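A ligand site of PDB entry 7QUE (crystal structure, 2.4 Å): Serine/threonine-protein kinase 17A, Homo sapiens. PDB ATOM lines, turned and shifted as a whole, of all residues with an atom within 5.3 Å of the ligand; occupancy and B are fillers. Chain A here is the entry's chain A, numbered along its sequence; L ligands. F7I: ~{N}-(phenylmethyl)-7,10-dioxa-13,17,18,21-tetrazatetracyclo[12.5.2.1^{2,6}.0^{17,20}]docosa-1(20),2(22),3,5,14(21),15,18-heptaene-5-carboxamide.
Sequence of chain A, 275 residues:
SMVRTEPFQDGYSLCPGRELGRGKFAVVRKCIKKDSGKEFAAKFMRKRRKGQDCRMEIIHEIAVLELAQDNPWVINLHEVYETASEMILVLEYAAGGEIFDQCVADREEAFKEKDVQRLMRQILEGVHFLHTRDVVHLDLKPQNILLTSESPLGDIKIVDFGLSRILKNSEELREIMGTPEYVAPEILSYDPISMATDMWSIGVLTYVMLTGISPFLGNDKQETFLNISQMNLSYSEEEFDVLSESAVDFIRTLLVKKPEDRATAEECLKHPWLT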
ATOM      1  N   LEU A  20     -10.427 -20.135   7.892  1.00  0.00           N
ATOM      2  CA  LEU A  20     -10.891 -20.048   6.520  1.00  0.00           C
ATOM      3  C   LEU A  20      -9.811 -19.518   5.576  1.00  0.00           C
ATOM      4  O   LEU A  20      -9.691 -20.006   4.450  1.00  0.00           O
ATOM      5  CB  LEU A  20     -12.147 -19.170   6.474  1.00  0.00           C
ATOM      6  CG  LEU A  20     -13.434 -19.757   7.079  1.00  0.00           C
ATOM      7  CD1 LEU A  20     -14.590 -18.788   6.887  1.00  0.00           C
ATOM      8  CD2 LEU A  20     -13.733 -21.123   6.453  1.00  0.00           C
ATOM      9  N   GLY A  21      -9.042 -18.538   6.005  1.00  0.00           N
ATOM     10  CA  GLY A  21      -7.988 -17.990   5.174  1.00  0.00           C
ATOM     11  C   GLY A  21      -7.032 -17.213   6.048  1.00  0.00           C
ATOM     12  O   GLY A  21      -7.410 -16.740   7.122  1.00  0.00           O
ATOM     13  N   ARG A  22      -5.786 -17.113   5.611  1.00  0.00           N
ATOM     14  CA  ARG A  22      -4.749 -16.426   6.365  1.00  0.00           C
ATOM     15  C   ARG A  22      -3.795 -15.715   5.418  1.00  0.00           C
ATOM     16  O   ARG A  22      -3.309 -16.307   4.451  1.00  0.00           O
ATOM     17  CB  ARG A  22      -3.973 -17.385   7.243  1.00  0.00           C
ATOM     18  CG  ARG A  22      -3.079 -16.690   8.238  1.00  0.00           C
ATOM     19  CD  ARG A  22      -2.445 -17.730   9.135  1.00  0.00           C
ATOM     20  NE  ARG A  22      -3.202 -17.917  10.379  1.00  0.00           N
ATOM     21  CZ  ARG A  22      -3.271 -17.024  11.362  1.00  0.00           C
ATOM     22  NH1 ARG A  22      -2.606 -15.887  11.323  1.00  0.00           N
ATOM     23  NH2 ARG A  22      -4.026 -17.305  12.435  1.00  0.00           N
ATOM     24  N   GLY A  23      -3.505 -14.454   5.720  1.00  0.00           N
ATOM     25  CA  GLY A  23      -2.630 -13.657   4.906  1.00  0.00           C
ATOM     26  C   GLY A  23      -1.653 -12.957   5.812  1.00  0.00           C
ATOM     27  O   GLY A  23      -1.632 -13.234   7.020  1.00  0.00           O
ATOM     28  N   LYS A  24      -0.856 -12.040   5.262  1.00  0.00           N
ATOM     29  CA  LYS A  24       0.202 -11.431   6.048  1.00  0.00           C
ATOM     30  C   LYS A  24      -0.358 -10.551   7.161  1.00  0.00           C
ATOM     31  O   LYS A  24       0.257 -10.446   8.220  1.00  0.00           O
ATOM     32  CB  LYS A  24       1.150 -10.637   5.151  1.00  0.00           C
ATOM     33  N   ALA A  26      -3.941 -10.545   8.104  1.00  0.00           N
ATOM     34  CA  ALA A  26      -5.335 -10.821   8.357  1.00  0.00           C
ATOM     35  C   ALA A  26      -5.559 -12.315   8.324  1.00  0.00           C
ATOM     36  O   ALA A  26      -4.826 -13.056   7.656  1.00  0.00           O
ATOM     37  CB  ALA A  26      -6.256 -10.118   7.330  1.00  0.00           C
ATOM     38  N   VAL A  27      -6.583 -12.760   9.058  1.00  0.00           N
ATOM     39  CA  VAL A  27      -7.013 -14.142   9.046  1.00  0.00           C
ATOM     40  C   VAL A  27      -8.536 -14.098   9.043  1.00  0.00           C
ATOM     41  O   VAL A  27      -9.146 -13.186   9.612  1.00  0.00           O
ATOM     42  CB  VAL A  27      -6.436 -14.947  10.249  1.00  0.00           C
ATOM     43  CG1 VAL A  27      -6.501 -14.138  11.495  1.00  0.00           C
ATOM     44  CG2 VAL A  27      -7.182 -16.275  10.467  1.00  0.00           C
ATOM     45  N   VAL A  28      -9.145 -15.058   8.357  1.00  0.00           N
ATOM     46  CA  VAL A  28     -10.590 -15.160   8.321  1.00  0.00           C
ATOM     47  C   VAL A  28     -10.998 -16.430   9.052  1.00  0.00           C
ATOM     48  O   VAL A  28     -10.481 -17.508   8.761  1.00  0.00           O
ATOM     49  CB  VAL A  28     -11.128 -15.177   6.872  1.00  0.00           C
ATOM     50  CG1 VAL A  28     -12.658 -15.082   6.908  1.00  0.00           C
ATOM     51  CG2 VAL A  28     -10.514 -14.061   6.061  1.00  0.00           C
ATOM     52  N   ALA A  41     -18.354 -14.975   8.339  1.00  0.00           N
ATOM     53  CA  ALA A  41     -16.910 -15.084   8.173  1.00  0.00           C
ATOM     54  C   ALA A  41     -16.268 -13.863   8.813  1.00  0.00           C
ATOM     55  O   ALA A  41     -16.408 -12.744   8.316  1.00  0.00           O
ATOM     56  CB  ALA A  41     -16.559 -15.190   6.690  1.00  0.00           C
ATOM     57  N   LYS A  43     -13.274 -11.550   9.623  1.00  0.00           N
ATOM     58  CA  LYS A  43     -11.962 -11.230   9.056  1.00  0.00           C
ATOM     59  C   LYS A  43     -11.203 -10.287   9.990  1.00  0.00           C
ATOM     60  O   LYS A  43     -11.496  -9.085  10.036  1.00  0.00           O
ATOM     61  CB  LYS A  43     -12.081 -10.612   7.670  1.00  0.00           C
ATOM     62  CG  LYS A  43     -10.741 -10.118   7.097  1.00  0.00           C
ATOM     63  CD  LYS A  43     -10.706 -10.198   5.604  1.00  0.00           C
ATOM     64  CE  LYS A  43      -9.402  -9.625   5.060  1.00  0.00           C
ATOM     65  NZ  LYS A  43      -9.703  -9.162   3.696  1.00  0.00           N
ATOM     66  N   GLU A  61     -10.761  -1.080   2.274  1.00  0.00           N
ATOM     67  CA  GLU A  61     -11.498  -2.320   2.019  1.00  0.00           C
ATOM     68  C   GLU A  61     -12.971  -2.191   2.381  1.00  0.00           C
ATOM     69  O   GLU A  61     -13.861  -2.581   1.618  1.00  0.00           O
ATOM     70  CB  GLU A  61     -10.840  -3.468   2.795  1.00  0.00           C
ATOM     71  CG  GLU A  61     -10.772  -4.761   2.012  1.00  0.00           C
ATOM     72  CD  GLU A  61      -9.911  -5.790   2.686  1.00  0.00           C
ATOM     73  OE1 GLU A  61      -8.678  -5.584   2.704  1.00  0.00           O
ATOM     74  OE2 GLU A  61     -10.474  -6.767   3.229  1.00  0.00           O
ATOM     75  N   ILE A  75     -19.576 -10.366  -1.842  1.00  0.00           N
ATOM     76  CA  ILE A  75     -19.730 -10.700  -0.433  1.00  0.00           C
ATOM     77  C   ILE A  75     -20.285  -9.504   0.356  1.00  0.00           C
ATOM     78  O   ILE A  75     -19.878  -8.345   0.164  1.00  0.00           O
ATOM     79  CB  ILE A  75     -18.359 -11.164   0.093  1.00  0.00           C
ATOM     80  CG1 ILE A  75     -18.476 -12.089   1.308  1.00  0.00           C
ATOM     81  CG2 ILE A  75     -17.387  -9.994   0.330  1.00  0.00           C
ATOM     82  CD1 ILE A  75     -19.071 -13.433   0.952  1.00  0.00           C
ATOM     83  N   LEU A  91     -18.142 -10.760   7.908  1.00  0.00           N
ATOM     84  CA  LEU A  91     -18.603 -10.894   6.532  1.00  0.00           C
ATOM     85  C   LEU A  91     -19.657 -11.970   6.401  1.00  0.00           C
ATOM     86  O   LEU A  91     -19.766 -12.876   7.233  1.00  0.00           O
ATOM     87  CB  LEU A  91     -17.450 -11.201   5.594  1.00  0.00           C
ATOM     88  CG  LEU A  91     -16.349 -10.142   5.527  1.00  0.00           C
ATOM     89  CD1 LEU A  91     -15.073 -10.695   4.884  1.00  0.00           C
ATOM     90  CD2 LEU A  91     -16.846  -8.908   4.769  1.00  0.00           C
ATOM     91  N   GLU A  92     -20.395 -11.885   5.305  1.00  0.00           N
ATOM     92  CA  GLU A  92     -21.304 -12.962   4.897  1.00  0.00           C
ATOM     93  C   GLU A  92     -20.526 -14.246   4.616  1.00  0.00           C
ATOM     94  O   GLU A  92     -19.419 -14.217   4.067  1.00  0.00           O
ATOM     95  CB  GLU A  92     -22.097 -12.544   3.652  1.00  0.00           C
ATOM     96  CG  GLU A  92     -22.764 -13.688   2.905  1.00  0.00           C
ATOM     97  CD  GLU A  92     -23.293 -13.232   1.533  1.00  0.00           C
ATOM     98  OE1 GLU A  92     -22.714 -12.303   0.920  1.00  0.00           O
ATOM     99  OE2 GLU A  92     -24.322 -13.783   1.076  1.00  0.00           O
ATOM    100  N   TYR A  93     -21.099 -15.369   5.031  1.00  0.00           N
ATOM    101  CA  TYR A  93     -20.469 -16.673   4.894  1.00  0.00           C
ATOM    102  C   TYR A  93     -20.965 -17.372   3.623  1.00  0.00           C
ATOM    103  O   TYR A  93     -22.169 -17.614   3.471  1.00  0.00           O
ATOM    104  CB  TYR A  93     -20.795 -17.508   6.130  1.00  0.00           C
ATOM    105  CG  TYR A  93     -20.269 -18.906   6.064  1.00  0.00           C
ATOM    106  CD1 TYR A  93     -18.893 -19.149   6.056  1.00  0.00           C
ATOM    107  CD2 TYR A  93     -21.140 -20.000   5.997  1.00  0.00           C
ATOM    108  CE1 TYR A  93     -18.381 -20.428   6.006  1.00  0.00           C
ATOM    109  CE2 TYR A  93     -20.623 -21.307   5.953  1.00  0.00           C
ATOM    110  CZ  TYR A  93     -19.245 -21.496   5.955  1.00  0.00           C
ATOM    111  OH  TYR A  93     -18.683 -22.756   5.914  1.00  0.00           O
ATOM    112  N   ALA A  94     -20.049 -17.747   2.747  1.00  0.00           N
ATOM    113  CA  ALA A  94     -20.410 -18.386   1.467  1.00  0.00           C
ATOM    114  C   ALA A  94     -20.154 -19.886   1.612  1.00  0.00           C
ATOM    115  O   ALA A  94     -19.012 -20.341   1.463  1.00  0.00           O
ATOM    116  CB  ALA A  94     -19.588 -17.807   0.319  1.00  0.00           C
ATOM    117  N   ALA A  95     -21.210 -20.670   1.905  1.00  0.00           N
ATOM    118  CA  ALA A  95     -20.993 -22.034   2.352  1.00  0.00           C
ATOM    119  C   ALA A  95     -20.260 -22.909   1.319  1.00  0.00           C
ATOM    120  O   ALA A  95     -19.745 -23.955   1.689  1.00  0.00           O
ATOM    121  CB  ALA A  95     -22.322 -22.707   2.754  1.00  0.00           C
ATOM    122  N   GLY A  97     -17.402 -22.219  -0.397  1.00  0.00           N
ATOM    123  CA  GLY A  97     -15.975 -22.169  -0.563  1.00  0.00           C
ATOM    124  C   GLY A  97     -15.543 -21.751  -1.960  1.00  0.00           C
ATOM    125  O   GLY A  97     -16.335 -21.283  -2.785  1.00  0.00           O
ATOM    126  N   GLU A  98     -14.247 -21.911  -2.209  1.00  0.00           N
ATOM    127  CA  GLU A  98     -13.635 -21.505  -3.472  1.00  0.00           C
ATOM    128  C   GLU A  98     -14.172 -22.311  -4.654  1.00  0.00           C
ATOM    129  O   GLU A  98     -14.507 -23.496  -4.508  1.00  0.00           O
ATOM    130  CB  GLU A  98     -12.142 -21.704  -3.441  1.00  0.00           C
ATOM    131  CG  GLU A  98     -11.388 -20.942  -2.424  1.00  0.00           C
ATOM    132  CD  GLU A  98      -9.991 -21.534  -2.293  1.00  0.00           C
ATOM    133  OE1 GLU A  98      -9.814 -22.669  -2.798  1.00  0.00           O
ATOM    134  OE2 GLU A  98      -9.075 -20.855  -1.753  1.00  0.00           O
ATOM    135  N   GLN A 143      -9.086 -18.448  -5.964  1.00  0.00           N
ATOM    136  CA  GLN A 143      -9.125 -18.288  -4.504  1.00  0.00           C
ATOM    137  C   GLN A 143     -10.156 -17.253  -4.060  1.00  0.00           C
ATOM    138  O   GLN A 143     -10.734 -17.364  -2.966  1.00  0.00           O
ATOM    139  CB  GLN A 143      -7.727 -17.894  -4.002  1.00  0.00           C
ATOM    140  CG  GLN A 143      -6.634 -18.990  -4.121  1.00  0.00           C
ATOM    141  CD  GLN A 143      -6.241 -19.324  -5.570  1.00  0.00           C
ATOM    142  OE1 GLN A 143      -6.557 -18.595  -6.519  1.00  0.00           O
ATOM    143  NE2 GLN A 143      -5.522 -20.444  -5.747  1.00  0.00           N
ATOM    144  N   ASN A 144     -10.421 -16.256  -4.897  1.00  0.00           N
ATOM    145  CA  ASN A 144     -11.274 -15.152  -4.532  1.00  0.00           C
ATOM    146  C   ASN A 144     -12.662 -15.209  -5.150  1.00  0.00           C
ATOM    147  O   ASN A 144     -13.397 -14.220  -5.058  1.00  0.00           O
ATOM    148  CB  ASN A 144     -10.617 -13.824  -4.882  1.00  0.00           C
ATOM    149  CG  ASN A 144      -9.496 -13.468  -3.961  1.00  0.00           C
ATOM    150  OD1 ASN A 144      -9.621 -13.616  -2.740  1.00  0.00           O
ATOM    151  ND2 ASN A 144      -8.420 -12.903  -4.512  1.00  0.00           N
ATOM    152  N   LEU A 146     -15.973 -17.224  -4.649  1.00  0.00           N
ATOM    153  CA  LEU A 146     -16.613 -18.211  -3.795  1.00  0.00           C
ATOM    154  C   LEU A 146     -17.962 -18.638  -4.357  1.00  0.00           C
ATOM    155  O   LEU A 146     -18.561 -17.976  -5.200  1.00  0.00           O
ATOM    156  CB  LEU A 146     -16.790 -17.680  -2.372  1.00  0.00           C
ATOM    157  CG  LEU A 146     -15.510 -17.138  -1.721  1.00  0.00           C
ATOM    158  CD1 LEU A 146     -15.754 -16.802  -0.220  1.00  0.00           C
ATOM    159  CD2 LEU A 146     -14.278 -18.077  -1.916  1.00  0.00           C
ATOM    160  N   VAL A 159     -14.843 -12.003  -3.307  1.00  0.00           N
ATOM    161  CA  VAL A 159     -14.297 -11.524  -2.046  1.00  0.00           C
ATOM    162  C   VAL A 159     -12.948 -10.864  -2.312  1.00  0.00           C
ATOM    163  O   VAL A 159     -12.389 -10.939  -3.404  1.00  0.00           O
ATOM    164  CB  VAL A 159     -14.151 -12.655  -1.000  1.00  0.00           C
ATOM    165  CG1 VAL A 159     -15.511 -13.319  -0.741  1.00  0.00           C
ATOM    166  CG2 VAL A 159     -13.082 -13.702  -1.429  1.00  0.00           C
ATOM    167  N   ASP A 160     -12.441 -10.189  -1.274  1.00  0.00           N
ATOM    168  CA  ASP A 160     -11.064  -9.725  -1.203  1.00  0.00           C
ATOM    169  C   ASP A 160     -10.791  -8.538  -2.104  1.00  0.00           C
ATOM    170  O   ASP A 160     -10.233  -8.671  -3.192  1.00  0.00           O
ATOM    171  CB  ASP A 160     -10.068 -10.831  -1.532  1.00  0.00           C
ATOM    172  CG  ASP A 160      -8.632 -10.371  -1.349  1.00  0.00           C
ATOM    173  OD1 ASP A 160      -8.413  -9.263  -0.768  1.00  0.00           O
ATOM    174  OD2 ASP A 160      -7.717 -11.139  -1.747  1.00  0.00           O
HETATM  175  C23 F7I L   1     -15.096 -17.640   3.107  1.00  0.00           C
HETATM  176  C19 F7I L   1     -15.675 -20.296   2.998  1.00  0.00           C
HETATM  177  C18 F7I L   1     -14.387 -19.755   2.737  1.00  0.00           C
HETATM  178  C17 F7I L   1     -11.950 -20.053   2.277  1.00  0.00           C
HETATM  179  C20 F7I L   1     -16.664 -19.416   3.253  1.00  0.00           C
HETATM  180  C21 F7I L   1     -16.519 -15.943   3.343  1.00  0.00           C
HETATM  181  C16 F7I L   1     -11.786 -19.396   0.933  1.00  0.00           C
HETATM  182  C13 F7I L   1     -11.961 -14.729   1.802  1.00  0.00           C
HETATM  183  C11 F7I L   1     -14.065 -15.255   2.841  1.00  0.00           C
HETATM  184  C12 F7I L   1     -12.943 -15.653   2.131  1.00  0.00           C
HETATM  185  C10 F7I L   1     -14.183 -13.922   3.225  1.00  0.00           C
HETATM  186  C6  F7I L   1      -7.153 -13.333   4.572  1.00  0.00           C
HETATM  187  C5  F7I L   1      -6.093 -12.472   4.760  1.00  0.00           C
HETATM  188  C1  F7I L   1      -8.616 -12.075   1.310  1.00  0.00           C
HETATM  189  C2  F7I L   1      -7.714 -12.234   2.500  1.00  0.00           C
HETATM  190  C3  F7I L   1      -6.634 -11.383   2.690  1.00  0.00           C
HETATM  191  O1  F7I L   1     -10.875 -15.036   1.035  1.00  0.00           O
HETATM  192  O2  F7I L   1     -10.606 -18.603   0.930  1.00  0.00           O
HETATM  193  C4  F7I L   1      -5.825 -11.500   3.813  1.00  0.00           C
HETATM  194  C7  F7I L   1      -7.963 -13.216   3.449  1.00  0.00           C
HETATM  195  N   F7I L   1      -9.828 -12.885   1.439  1.00  0.00           N
HETATM  196  C   F7I L   1     -10.958 -12.396   1.956  1.00  0.00           C
HETATM  197  O   F7I L   1     -11.098 -11.197   2.238  1.00  0.00           O
HETATM  198  C14 F7I L   1     -10.236 -16.293   1.263  1.00  0.00           C
HETATM  199  C15 F7I L   1     -10.791 -17.329   0.330  1.00  0.00           C
HETATM  200  C22 F7I L   1     -15.159 -16.225   3.123  1.00  0.00           C
HETATM  201  C8  F7I L   1     -12.049 -13.393   2.205  1.00  0.00           C
HETATM  202  C9  F7I L   1     -13.179 -13.013   2.911  1.00  0.00           C
HETATM  203  N1  F7I L   1     -13.299 -20.568   2.471  1.00  0.00           N
HETATM  204  N2  F7I L   1     -16.371 -18.085   3.286  1.00  0.00           N
HETATM  205  N3  F7I L   1     -17.272 -17.035   3.429  1.00  0.00           N
HETATM  206  N4  F7I L   1     -14.118 -18.437   2.693  1.00  0.00           N
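A nitrogen (N3) of the ligand is in hydrogen-bond range of the backbone NH (N) of Ala 94 (2.9 Å). O of the ligand sits at hydrogen-bond distance from NZ of Lys 43 (2.9 Å).
The side-chain amino group (NZ) of Lys 43 is in salt-bridge range of the side-chain carboxylate (OE2) of Glu 61 (2.6 Å). The backbone carbonyl oxygen (O) of Ala 41 lies within hydrogen-bond range of the backbone NH (N) of Leu 91, 2.7 Å away. The backbone NH of Val 159 lies within hydrogen-bond range of the backbone carbonyl oxygen of Asn 144, at 3.2 Å. The backbone carbonyl oxygen (O) of Val 28 sits at hydrogen-bond distance from the backbone NH (N) of Leu 20, 2.8 Å away. The side-chain carboxylate (OD2) of Asp 160 sits close to the side-chain amide oxygen (OD1) of Asn 144. N of Val 28 sits at hydrogen-bond distance from O of Gly 21 (2.7 Å).
Residues that only touch the ligand: Leu 20 (3.1 Å), Asp 160 (3.2 Å), Ala 26 (3.2 Å), Gln 143 (3.3 Å), Gly 23 (3.4 Å), Tyr 93 (3.4 Å), Ala 41 (3.4 Å), Leu 146 (3.4 Å), Glu 92 (3.5 Å), Val 159 (3.6 Å), Leu 91 (3.6 Å), Glu 98 (3.7 Å) and Val 28 (3.7 Å). Hydrophobic or aromatic side chains within 4 Å of the ligand: Leu 20, Ala 26, Val 28, Ala 41, Leu 91, Tyr 93, Ala 94, Leu 146 and Val 159. Within 4 Å of the ligand: Leu 20, Gly 23, Ala 26, Val 28, Ala 41, Lys 43, Leu 91, Glu 92, Tyr 93, Ala 94, Glu 98, Gln 143, Leu 146, Val 159 and Asp 160.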
